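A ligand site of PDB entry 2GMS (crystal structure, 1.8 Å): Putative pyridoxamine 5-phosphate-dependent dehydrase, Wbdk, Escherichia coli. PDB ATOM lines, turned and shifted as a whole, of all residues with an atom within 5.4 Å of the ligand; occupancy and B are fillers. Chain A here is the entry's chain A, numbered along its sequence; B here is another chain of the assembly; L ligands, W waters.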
ATOM      1  N   SER A  57      29.180   0.385 -13.470  1.00  0.00           N
ATOM      2  CA  SER A  57      28.297  -0.662 -12.995  1.00  0.00           C
ATOM      3  C   SER A  57      28.896  -2.035 -13.298  1.00  0.00           C
ATOM      4  O   SER A  57      29.848  -2.193 -14.080  1.00  0.00           O
ATOM      5  CB  SER A  57      26.867  -0.608 -13.599  1.00  0.00           C
ATOM      6  OG  SER A  57      26.877  -0.684 -15.030  1.00  0.00           O
ATOM      7  N   GLY A  58      28.299  -3.036 -12.692  1.00  0.00           N
ATOM      8  CA  GLY A  58      28.730  -4.384 -12.975  1.00  0.00           C
ATOM      9  C   GLY A  58      28.320  -4.655 -14.424  1.00  0.00           C
ATOM     10  O   GLY A  58      28.977  -5.397 -15.130  1.00  0.00           O
ATOM     11  N   SER A  59      27.239  -4.009 -14.896  1.00  0.00           N
ATOM     12  CA  SER A  59      26.793  -4.210 -16.275  1.00  0.00           C
ATOM     13  C   SER A  59      27.794  -3.693 -17.295  1.00  0.00           C
ATOM     14  O   SER A  59      28.023  -4.282 -18.346  1.00  0.00           O
ATOM     15  CB  SER A  59      25.437  -3.550 -16.542  1.00  0.00           C
ATOM     16  OG  SER A  59      24.458  -4.264 -15.837  1.00  0.00           O
ATOM     17  N   THR A  60      28.389  -2.550 -17.017  1.00  0.00           N
ATOM     18  CA  THR A  60      29.386  -1.999 -17.944  1.00  0.00           C
ATOM     19  C   THR A  60      30.716  -2.731 -17.762  1.00  0.00           C
ATOM     20  O   THR A  60      31.565  -2.723 -18.666  1.00  0.00           O
ATOM     21  CB  THR A  60      29.565  -0.470 -17.860  1.00  0.00           C
ATOM     22  OG1 THR A  60      29.882  -0.128 -16.523  1.00  0.00           O
ATOM     23  CG2 THR A  60      28.293   0.279 -18.340  1.00  0.00           C
ATOM     24  N   ASN A  62      30.921  -5.976 -17.495  1.00  0.00           N
ATOM     25  CA  ASN A  62      30.665  -7.089 -18.419  1.00  0.00           C
ATOM     26  C   ASN A  62      30.872  -6.673 -19.880  1.00  0.00           C
ATOM     27  O   ASN A  62      31.451  -7.391 -20.687  1.00  0.00           O
ATOM     28  CB  ASN A  62      29.217  -7.636 -18.257  1.00  0.00           C
ATOM     29  CG  ASN A  62      29.009  -8.620 -17.135  1.00  0.00           C
ATOM     30  OD1 ASN A  62      29.991  -9.046 -16.494  1.00  0.00           O
ATOM     31  ND2 ASN A  62      27.764  -9.056 -16.890  1.00  0.00           N
ATOM     32  N   SER A  89      21.096 -16.361 -15.267  1.00  0.00           N
ATOM     33  CA  SER A  89      21.976 -15.259 -14.920  1.00  0.00           C
ATOM     34  C   SER A  89      21.236 -13.927 -15.028  1.00  0.00           C
ATOM     35  O   SER A  89      20.044 -13.892 -15.315  1.00  0.00           O
ATOM     36  CB  SER A  89      23.232 -15.244 -15.791  1.00  0.00           C
ATOM     37  OG  SER A  89      24.034 -14.215 -15.235  1.00  0.00           O
ATOM     38  N   TRP A  90      21.931 -12.820 -14.867  1.00  0.00           N
ATOM     39  CA  TRP A  90      21.306 -11.517 -15.003  1.00  0.00           C
ATOM     40  C   TRP A  90      21.256 -11.148 -16.499  1.00  0.00           C
ATOM     41  O   TRP A  90      22.057 -11.615 -17.283  1.00  0.00           O
ATOM     42  CB  TRP A  90      22.037 -10.462 -14.150  1.00  0.00           C
ATOM     43  CG  TRP A  90      21.367  -9.121 -14.229  1.00  0.00           C
ATOM     44  CD1 TRP A  90      21.853  -8.005 -14.837  1.00  0.00           C
ATOM     45  CD2 TRP A  90      20.077  -8.803 -13.743  1.00  0.00           C
ATOM     46  NE1 TRP A  90      20.920  -7.005 -14.743  1.00  0.00           N
ATOM     47  CE2 TRP A  90      19.825  -7.458 -14.080  1.00  0.00           C
ATOM     48  CE3 TRP A  90      19.106  -9.539 -13.060  1.00  0.00           C
ATOM     49  CZ2 TRP A  90      18.618  -6.829 -13.760  1.00  0.00           C
ATOM     50  CZ3 TRP A  90      17.919  -8.909 -12.730  1.00  0.00           C
ATOM     51  CH2 TRP A  90      17.678  -7.564 -13.058  1.00  0.00           C
ATOM     52  N   THR A  92      22.285  -8.628 -18.184  1.00  0.00           N
ATOM     53  CA  THR A  92      23.492  -7.989 -18.674  1.00  0.00           C
ATOM     54  C   THR A  92      24.695  -8.886 -18.764  1.00  0.00           C
ATOM     55  O   THR A  92      25.801  -8.465 -19.121  1.00  0.00           O
ATOM     56  CB  THR A  92      23.837  -6.637 -18.050  1.00  0.00           C
ATOM     57  OG1 THR A  92      23.949  -6.766 -16.639  1.00  0.00           O
ATOM     58  CG2 THR A  92      22.806  -5.601 -18.493  1.00  0.00           C
ATOM     59  N   THR A  93      24.496 -10.135 -18.462  1.00  0.00           N
ATOM     60  CA  THR A  93      25.583 -11.054 -18.636  1.00  0.00           C
ATOM     61  C   THR A  93      25.557 -11.398 -20.141  1.00  0.00           C
ATOM     62  O   THR A  93      26.575 -11.611 -20.791  1.00  0.00           O
ATOM     63  CB  THR A  93      25.292 -12.331 -17.827  1.00  0.00           C
ATOM     64  OG1 THR A  93      25.271 -12.057 -16.448  1.00  0.00           O
ATOM     65  CG2 THR A  93      26.251 -13.455 -18.147  1.00  0.00           C
ATOM     66  N   VAL A 135      29.304 -17.983 -14.544  1.00  0.00           N
ATOM     67  CA  VAL A 135      28.640 -17.078 -13.629  1.00  0.00           C
ATOM     68  C   VAL A 135      28.636 -17.750 -12.266  1.00  0.00           C
ATOM     69  O   VAL A 135      28.238 -18.890 -12.157  1.00  0.00           O
ATOM     70  CB  VAL A 135      27.213 -16.757 -14.133  1.00  0.00           C
ATOM     71  CG1 VAL A 135      26.401 -15.956 -13.138  1.00  0.00           C
ATOM     72  CG2 VAL A 135      27.217 -16.053 -15.492  1.00  0.00           C
ATOM     73  N   ASP A 161      31.606 -13.895 -14.575  1.00  0.00           N
ATOM     74  CA  ASP A 161      30.725 -12.828 -14.158  1.00  0.00           C
ATOM     75  C   ASP A 161      30.605 -13.130 -12.655  1.00  0.00           C
ATOM     76  O   ASP A 161      29.943 -14.101 -12.271  1.00  0.00           O
ATOM     77  CB  ASP A 161      29.348 -12.830 -14.848  1.00  0.00           C
ATOM     78  CG  ASP A 161      28.393 -11.812 -14.268  1.00  0.00           C
ATOM     79  OD1 ASP A 161      28.489 -11.387 -13.110  1.00  0.00           O
ATOM     80  OD2 ASP A 161      27.445 -11.436 -15.113  1.00  0.00           O
ATOM     81  N   CYS A 163      29.514 -10.912 -10.334  1.00  0.00           N
ATOM     82  CA  CYS A 163      28.650  -9.874  -9.799  1.00  0.00           C
ATOM     83  C   CYS A 163      27.845 -10.242  -8.568  1.00  0.00           C
ATOM     84  O   CYS A 163      27.373  -9.359  -7.874  1.00  0.00           O
ATOM     85  CB  CYS A 163      27.793  -9.177 -10.872  1.00  0.00           C
ATOM     86  SG  CYS A 163      28.856  -8.232 -11.980  1.00  0.00           S
ATOM     87  N   GLU A 164      27.682 -11.540  -8.260  1.00  0.00           N
ATOM     88  CA  GLU A 164      26.925 -11.983  -7.079  1.00  0.00           C
ATOM     89  C   GLU A 164      27.777 -12.725  -6.059  1.00  0.00           C
ATOM     90  O   GLU A 164      27.290 -13.082  -4.982  1.00  0.00           O
ATOM     91  CB  GLU A 164      25.793 -12.956  -7.459  1.00  0.00           C
ATOM     92  CG  GLU A 164      24.716 -12.280  -8.339  1.00  0.00           C
ATOM     93  CD  GLU A 164      23.683 -13.248  -8.872  1.00  0.00           C
ATOM     94  OE1 GLU A 164      23.675 -14.439  -8.578  1.00  0.00           O
ATOM     95  OE2 GLU A 164      22.821 -12.692  -9.689  1.00  0.00           O
ATOM     96  N   SER A 185      30.190  -6.343  -9.011  1.00  0.00           N
ATOM     97  CA  SER A 185      29.205  -5.279  -8.915  1.00  0.00           C
ATOM     98  C   SER A 185      29.173  -4.749  -7.494  1.00  0.00           C
ATOM     99  O   SER A 185      29.237  -5.521  -6.539  1.00  0.00           O
ATOM    100  CB  SER A 185      27.830  -5.764  -9.341  1.00  0.00           C
ATOM    101  OG  SER A 185      26.810  -4.847  -8.955  1.00  0.00           O
ATOM    102  N   SER A 186      29.102  -3.423  -7.386  1.00  0.00           N
ATOM    103  CA  SER A 186      28.993  -2.738  -6.117  1.00  0.00           C
ATOM    104  C   SER A 186      27.711  -1.920  -6.066  1.00  0.00           C
ATOM    105  O   SER A 186      27.596  -0.865  -5.446  1.00  0.00           O
ATOM    106  CB  SER A 186      30.215  -1.947  -5.732  1.00  0.00           C
ATOM    107  OG  SER A 186      30.374  -0.866  -6.637  1.00  0.00           O
ATOM    108  N   PHE A 187      26.713  -2.437  -6.751  1.00  0.00           N
ATOM    109  CA  PHE A 187      25.431  -1.774  -6.738  1.00  0.00           C
ATOM    110  C   PHE A 187      24.788  -2.006  -5.363  1.00  0.00           C
ATOM    111  O   PHE A 187      25.195  -2.905  -4.618  1.00  0.00           O
ATOM    112  CB  PHE A 187      24.523  -2.393  -7.812  1.00  0.00           C
ATOM    113  CG  PHE A 187      23.136  -1.794  -7.816  1.00  0.00           C
ATOM    114  CD1 PHE A 187      22.957  -0.473  -8.217  1.00  0.00           C
ATOM    115  CD2 PHE A 187      22.017  -2.529  -7.447  1.00  0.00           C
ATOM    116  CE1 PHE A 187      21.674   0.099  -8.235  1.00  0.00           C
ATOM    117  CE2 PHE A 187      20.732  -1.981  -7.464  1.00  0.00           C
ATOM    118  CZ  PHE A 187      20.561  -0.653  -7.852  1.00  0.00           C
ATOM    119  N   HIS A 190      24.713  -5.283  -2.699  1.00  0.00           N
ATOM    120  CA  HIS A 190      25.584  -6.358  -3.085  1.00  0.00           C
ATOM    121  C   HIS A 190      26.475  -6.593  -1.881  1.00  0.00           C
ATOM    122  O   HIS A 190      26.157  -6.053  -0.843  1.00  0.00           O
ATOM    123  CB  HIS A 190      26.373  -5.939  -4.336  1.00  0.00           C
ATOM    124  CG  HIS A 190      25.485  -6.196  -5.489  1.00  0.00           C
ATOM    125  ND1 HIS A 190      25.801  -7.122  -6.483  1.00  0.00           N
ATOM    126  CD2 HIS A 190      24.242  -5.691  -5.742  1.00  0.00           C
ATOM    127  CE1 HIS A 190      24.768  -7.127  -7.327  1.00  0.00           C
ATOM    128  NE2 HIS A 190      23.810  -6.274  -6.911  1.00  0.00           N
ATOM    129  N   GLU A 196      26.242   2.884  -7.183  1.00  0.00           N
ATOM    130  CA  GLU A 196      26.350   2.105  -8.406  1.00  0.00           C
ATOM    131  C   GLU A 196      27.815   1.828  -8.573  1.00  0.00           C
ATOM    132  O   GLU A 196      28.635   2.621  -8.117  1.00  0.00           O
ATOM    133  CB  GLU A 196      25.810   2.759  -9.713  1.00  0.00           C
ATOM    134  CG  GLU A 196      24.280   2.926  -9.700  1.00  0.00           C
ATOM    135  CD  GLU A 196      23.558   2.087 -10.720  1.00  0.00           C
ATOM    136  OE1 GLU A 196      24.023   1.075 -11.229  1.00  0.00           O
ATOM    137  OE2 GLU A 196      22.379   2.593 -11.002  1.00  0.00           O
ATOM    138  N   GLY A 197      28.167   0.728  -9.219  1.00  0.00           N
ATOM    139  CA  GLY A 197      29.569   0.487  -9.407  1.00  0.00           C
ATOM    140  C   GLY A 197      29.869  -0.922  -9.868  1.00  0.00           C
ATOM    141  O   GLY A 197      29.100  -1.875  -9.640  1.00  0.00           O
ATOM    142  N   PHE A 304      25.113 -14.788  -1.226  1.00  0.00           N
ATOM    143  CA  PHE A 304      24.489 -13.556  -1.594  1.00  0.00           C
ATOM    144  C   PHE A 304      23.069 -13.553  -1.060  1.00  0.00           C
ATOM    145  O   PHE A 304      22.571 -12.570  -0.538  1.00  0.00           O
ATOM    146  CB  PHE A 304      24.473 -13.512  -3.121  1.00  0.00           C
ATOM    147  CG  PHE A 304      23.867 -12.254  -3.667  1.00  0.00           C
ATOM    148  CD1 PHE A 304      24.623 -11.089  -3.719  1.00  0.00           C
ATOM    149  CD2 PHE A 304      22.551 -12.211  -4.123  1.00  0.00           C
ATOM    150  CE1 PHE A 304      24.085  -9.912  -4.243  1.00  0.00           C
ATOM    151  CE2 PHE A 304      21.995 -11.044  -4.617  1.00  0.00           C
ATOM    152  CZ  PHE A 304      22.776  -9.891  -4.699  1.00  0.00           C
ATOM    153  N   ARG A 333      11.922 -13.147  -3.977  1.00  0.00           N
ATOM    154  CA  ARG A 333      12.258 -12.774  -5.428  1.00  0.00           C
ATOM    155  C   ARG A 333      12.349 -14.159  -6.175  1.00  0.00           C
ATOM    156  O   ARG A 333      12.477 -15.252  -5.563  1.00  0.00           O
ATOM    157  CB  ARG A 333      13.584 -11.803  -5.470  1.00  0.00           C
ATOM    158  CG  ARG A 333      14.603 -12.134  -6.561  1.00  0.00           C
ATOM    159  CD  ARG A 333      15.914 -11.329  -6.445  1.00  0.00           C
ATOM    160  NE  ARG A 333      16.500 -11.087  -7.764  1.00  0.00           N
ATOM    161  CZ  ARG A 333      17.432 -10.180  -8.022  1.00  0.00           C
ATOM    162  NH1 ARG A 333      17.671  -9.169  -7.164  1.00  0.00           N
ATOM    163  NH2 ARG A 333      18.175 -10.211  -9.131  1.00  0.00           N
ATOM    164  N   VAL A 336      17.162 -14.886  -9.422  1.00  0.00           N
ATOM    165  CA  VAL A 336      17.714 -14.027 -10.431  1.00  0.00           C
ATOM    166  C   VAL A 336      16.598 -13.766 -11.442  1.00  0.00           C
ATOM    167  O   VAL A 336      15.531 -13.280 -11.093  1.00  0.00           O
ATOM    168  CB  VAL A 336      19.061 -14.577 -10.998  1.00  0.00           C
ATOM    169  CG1 VAL A 336      19.839 -13.559 -11.817  1.00  0.00           C
ATOM    170  CG2 VAL A 336      19.983 -15.059  -9.889  1.00  0.00           C
ATOM    171  N   HIS B 217      18.923  -2.326 -18.036  1.00  0.00           N
ATOM    172  CA  HIS B 217      18.801  -3.768 -18.163  1.00  0.00           C
ATOM    173  C   HIS B 217      17.906  -4.331 -19.247  1.00  0.00           C
ATOM    174  O   HIS B 217      17.838  -5.556 -19.348  1.00  0.00           O
ATOM    175  CB  HIS B 217      18.431  -4.413 -16.801  1.00  0.00           C
ATOM    176  CG  HIS B 217      19.292  -3.879 -15.683  1.00  0.00           C
ATOM    177  ND1 HIS B 217      20.570  -4.355 -15.509  1.00  0.00           N
ATOM    178  CD2 HIS B 217      19.058  -2.913 -14.735  1.00  0.00           C
ATOM    179  CE1 HIS B 217      21.091  -3.708 -14.454  1.00  0.00           C
ATOM    180  NE2 HIS B 217      20.217  -2.831 -13.981  1.00  0.00           N
ATOM    181  N   ASN B 250      23.200  -0.919 -18.667  1.00  0.00           N
ATOM    182  CA  ASN B 250      22.958  -0.315 -17.376  1.00  0.00           C
ATOM    183  C   ASN B 250      23.737   1.008 -17.469  1.00  0.00           C
ATOM    184  O   ASN B 250      24.951   1.047 -17.294  1.00  0.00           O
ATOM    185  CB  ASN B 250      23.197  -1.081 -16.052  1.00  0.00           C
ATOM    186  CG  ASN B 250      23.114  -0.149 -14.839  1.00  0.00           C
ATOM    187  OD1 ASN B 250      22.734   1.047 -14.919  1.00  0.00           O
ATOM    188  ND2 ASN B 250      23.427  -0.707 -13.671  1.00  0.00           N
ATOM    189  N   ARG B 252      22.253   3.975 -16.096  1.00  0.00           N
ATOM    190  CA  ARG B 252      21.487   4.840 -15.243  1.00  0.00           C
ATOM    191  C   ARG B 252      22.391   5.904 -14.617  1.00  0.00           C
ATOM    192  O   ARG B 252      23.557   5.625 -14.329  1.00  0.00           O
ATOM    193  CB  ARG B 252      20.944   4.005 -14.113  1.00  0.00           C
ATOM    194  CG  ARG B 252      19.780   3.166 -14.527  1.00  0.00           C
ATOM    195  CD  ARG B 252      19.193   2.612 -13.241  1.00  0.00           C
ATOM    196  NE  ARG B 252      20.233   1.848 -12.586  1.00  0.00           N
ATOM    197  CZ  ARG B 252      20.024   0.667 -12.030  1.00  0.00           C
ATOM    198  NH1 ARG B 252      18.812   0.124 -12.015  1.00  0.00           N
ATOM    199  NH2 ARG B 252      21.052   0.014 -11.488  1.00  0.00           N
HETATM  200  O1  LIG L   1      23.621 -10.431 -10.802  1.00  0.00           O
HETATM  201  N1  LIG L   1      25.651  -9.873 -13.674  1.00  0.00           N
HETATM  202  C1  LIG L   1      25.008 -10.514 -12.720  1.00  0.00           C
HETATM  203  C2  LIG L   1      25.088 -12.020 -12.602  1.00  0.00           C
HETATM  204  C3  LIG L   1      24.271  -9.807 -11.810  1.00  0.00           C
HETATM  205  C4  LIG L   1      24.218  -8.419 -11.907  1.00  0.00           C
HETATM  206  C5  LIG L   1      23.433  -7.641 -10.871  1.00  0.00           C
HETATM  207  O2  LIG L   1      23.223  -8.461  -9.751  1.00  0.00           O
HETATM  208  O3  LIG L   1      22.208  -7.226 -11.377  1.00  0.00           O
HETATM  209  C6  LIG L   1      24.841  -7.736 -12.984  1.00  0.00           C
HETATM  210  C7  LIG L   1      25.595  -8.538 -13.807  1.00  0.00           C
HETATM  211  C8  LIG L   1      24.794  -6.385 -12.911  1.00  0.00           C
HETATM  212  O4  LIG L   1      25.503  -5.545 -12.110  1.00  0.00           O
HETATM  213  P1  LIG L   1      24.898  -4.062 -12.077  1.00  0.00           P
HETATM  214  O5  LIG L   1      23.546  -4.173 -11.503  1.00  0.00           O
HETATM  215  O6  LIG L   1      25.873  -3.254 -11.078  1.00  0.00           O
HETATM  216  O7  LIG L   1      24.861  -3.354 -13.518  1.00  0.00           O
HETATM  217  O   HOH W   1      21.317  -2.993 -10.932  1.00  0.00           O
HETATM  218  O   HOH W   2      21.592  -5.909  -9.382  1.00  0.00           O
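An oxygen (O7) of the ligand sits at hydrogen-bond distance from the backbone NH (N) of Ser 59, 2.8 Å away.
OG of Ser 59 lies within hydrogen-bond range of O7 of the ligand (2.5 Å).
The side-chain carboxylate of Glu 164 sits at hydrogen-bond distance from an oxygen (O1) of the ligand (2.6 Å).
OD2 of Asp 161 is in hydrogen-bond range of N1 of the ligand, 2.8 Å away.
OG of Ser 185 sits at hydrogen-bond distance from O6 of the ligand (2.8 Å).
The backbone NH (N) of Gly 58 is in hydrogen-bond range of an oxygen (O6) of the ligand (2.9 Å).
ND2 of Asn 250 of chain B sits at hydrogen-bond distance from O7 of the ligand (3.0 Å).
The side-chain hydroxyl (OG1) of Thr 92 lies within hydrogen-bond range of the side-chain hydroxyl (OG) of Ser 59 (2.7 Å).
OD1 of Asp 161 is in hydrogen-bond range of N of Cys 163 (3.0 Å).
The side-chain carboxylate of Asp 161 is in hydrogen-bond range of the side-chain amide nitrogen of Asn 62, at 3.0 Å.
OG of Ser 185 is in hydrogen-bond range of N of Phe 187, at 3.3 Å.
N of Gly 58 is in hydrogen-bond range of O of Gly 197, 3.4 Å away.
The side-chain amide oxygen (OD1) of Asn 250 of chain B lies within hydrogen-bond range of the backbone NH (N) of Arg 252 of chain B (3.2 Å).
The side-chain hydroxyl of Thr 93 lies within hydrogen-bond range of the side-chain hydroxyl of Ser 89, at 2.8 Å.
The backbone carbonyl oxygen (O) of Thr 92 is in hydrogen-bond range of the side-chain amide nitrogen (ND2) of Asn 62, 3.0 Å away.
Merely in contact with the ligand: Ser 57, Asn 62, Ser 89, Trp 90, Thr 92, Thr 93, Cys 163, Phe 187, His 190, Gly 197 and His 217 of chain B.
Hydrophobic or aromatic side chains that line the ligand: Trp 90, Phe 187, His 190 and His 217 of chain B.
17 residues have an atom within 4 Å of the ligand: Ser 57, Gly 58, Ser 59, Asn 62, Ser 89, Trp 90, Thr 92, Thr 93, Asp 161, Cys 163, Glu 164, Ser 185, Phe 187, His 190, Gly 197, His 217 of chain B and Asn 250 of chain B.
Along chain A the residues within 4 Å of the ligand span positions 57 to 197.
The nearest printed residue that does not touch the ligand is Val 135 (4.2 Å).
Water W2 bridges O3 of the ligand and NE2 of His 190.
Water W1 lies within hydrogen-bond range of O5 of the ligand (2.6 Å), NH2 of Arg 252 of chain B (3.1 Å) and NE2 of His 217 of chain B (3.2 Å).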
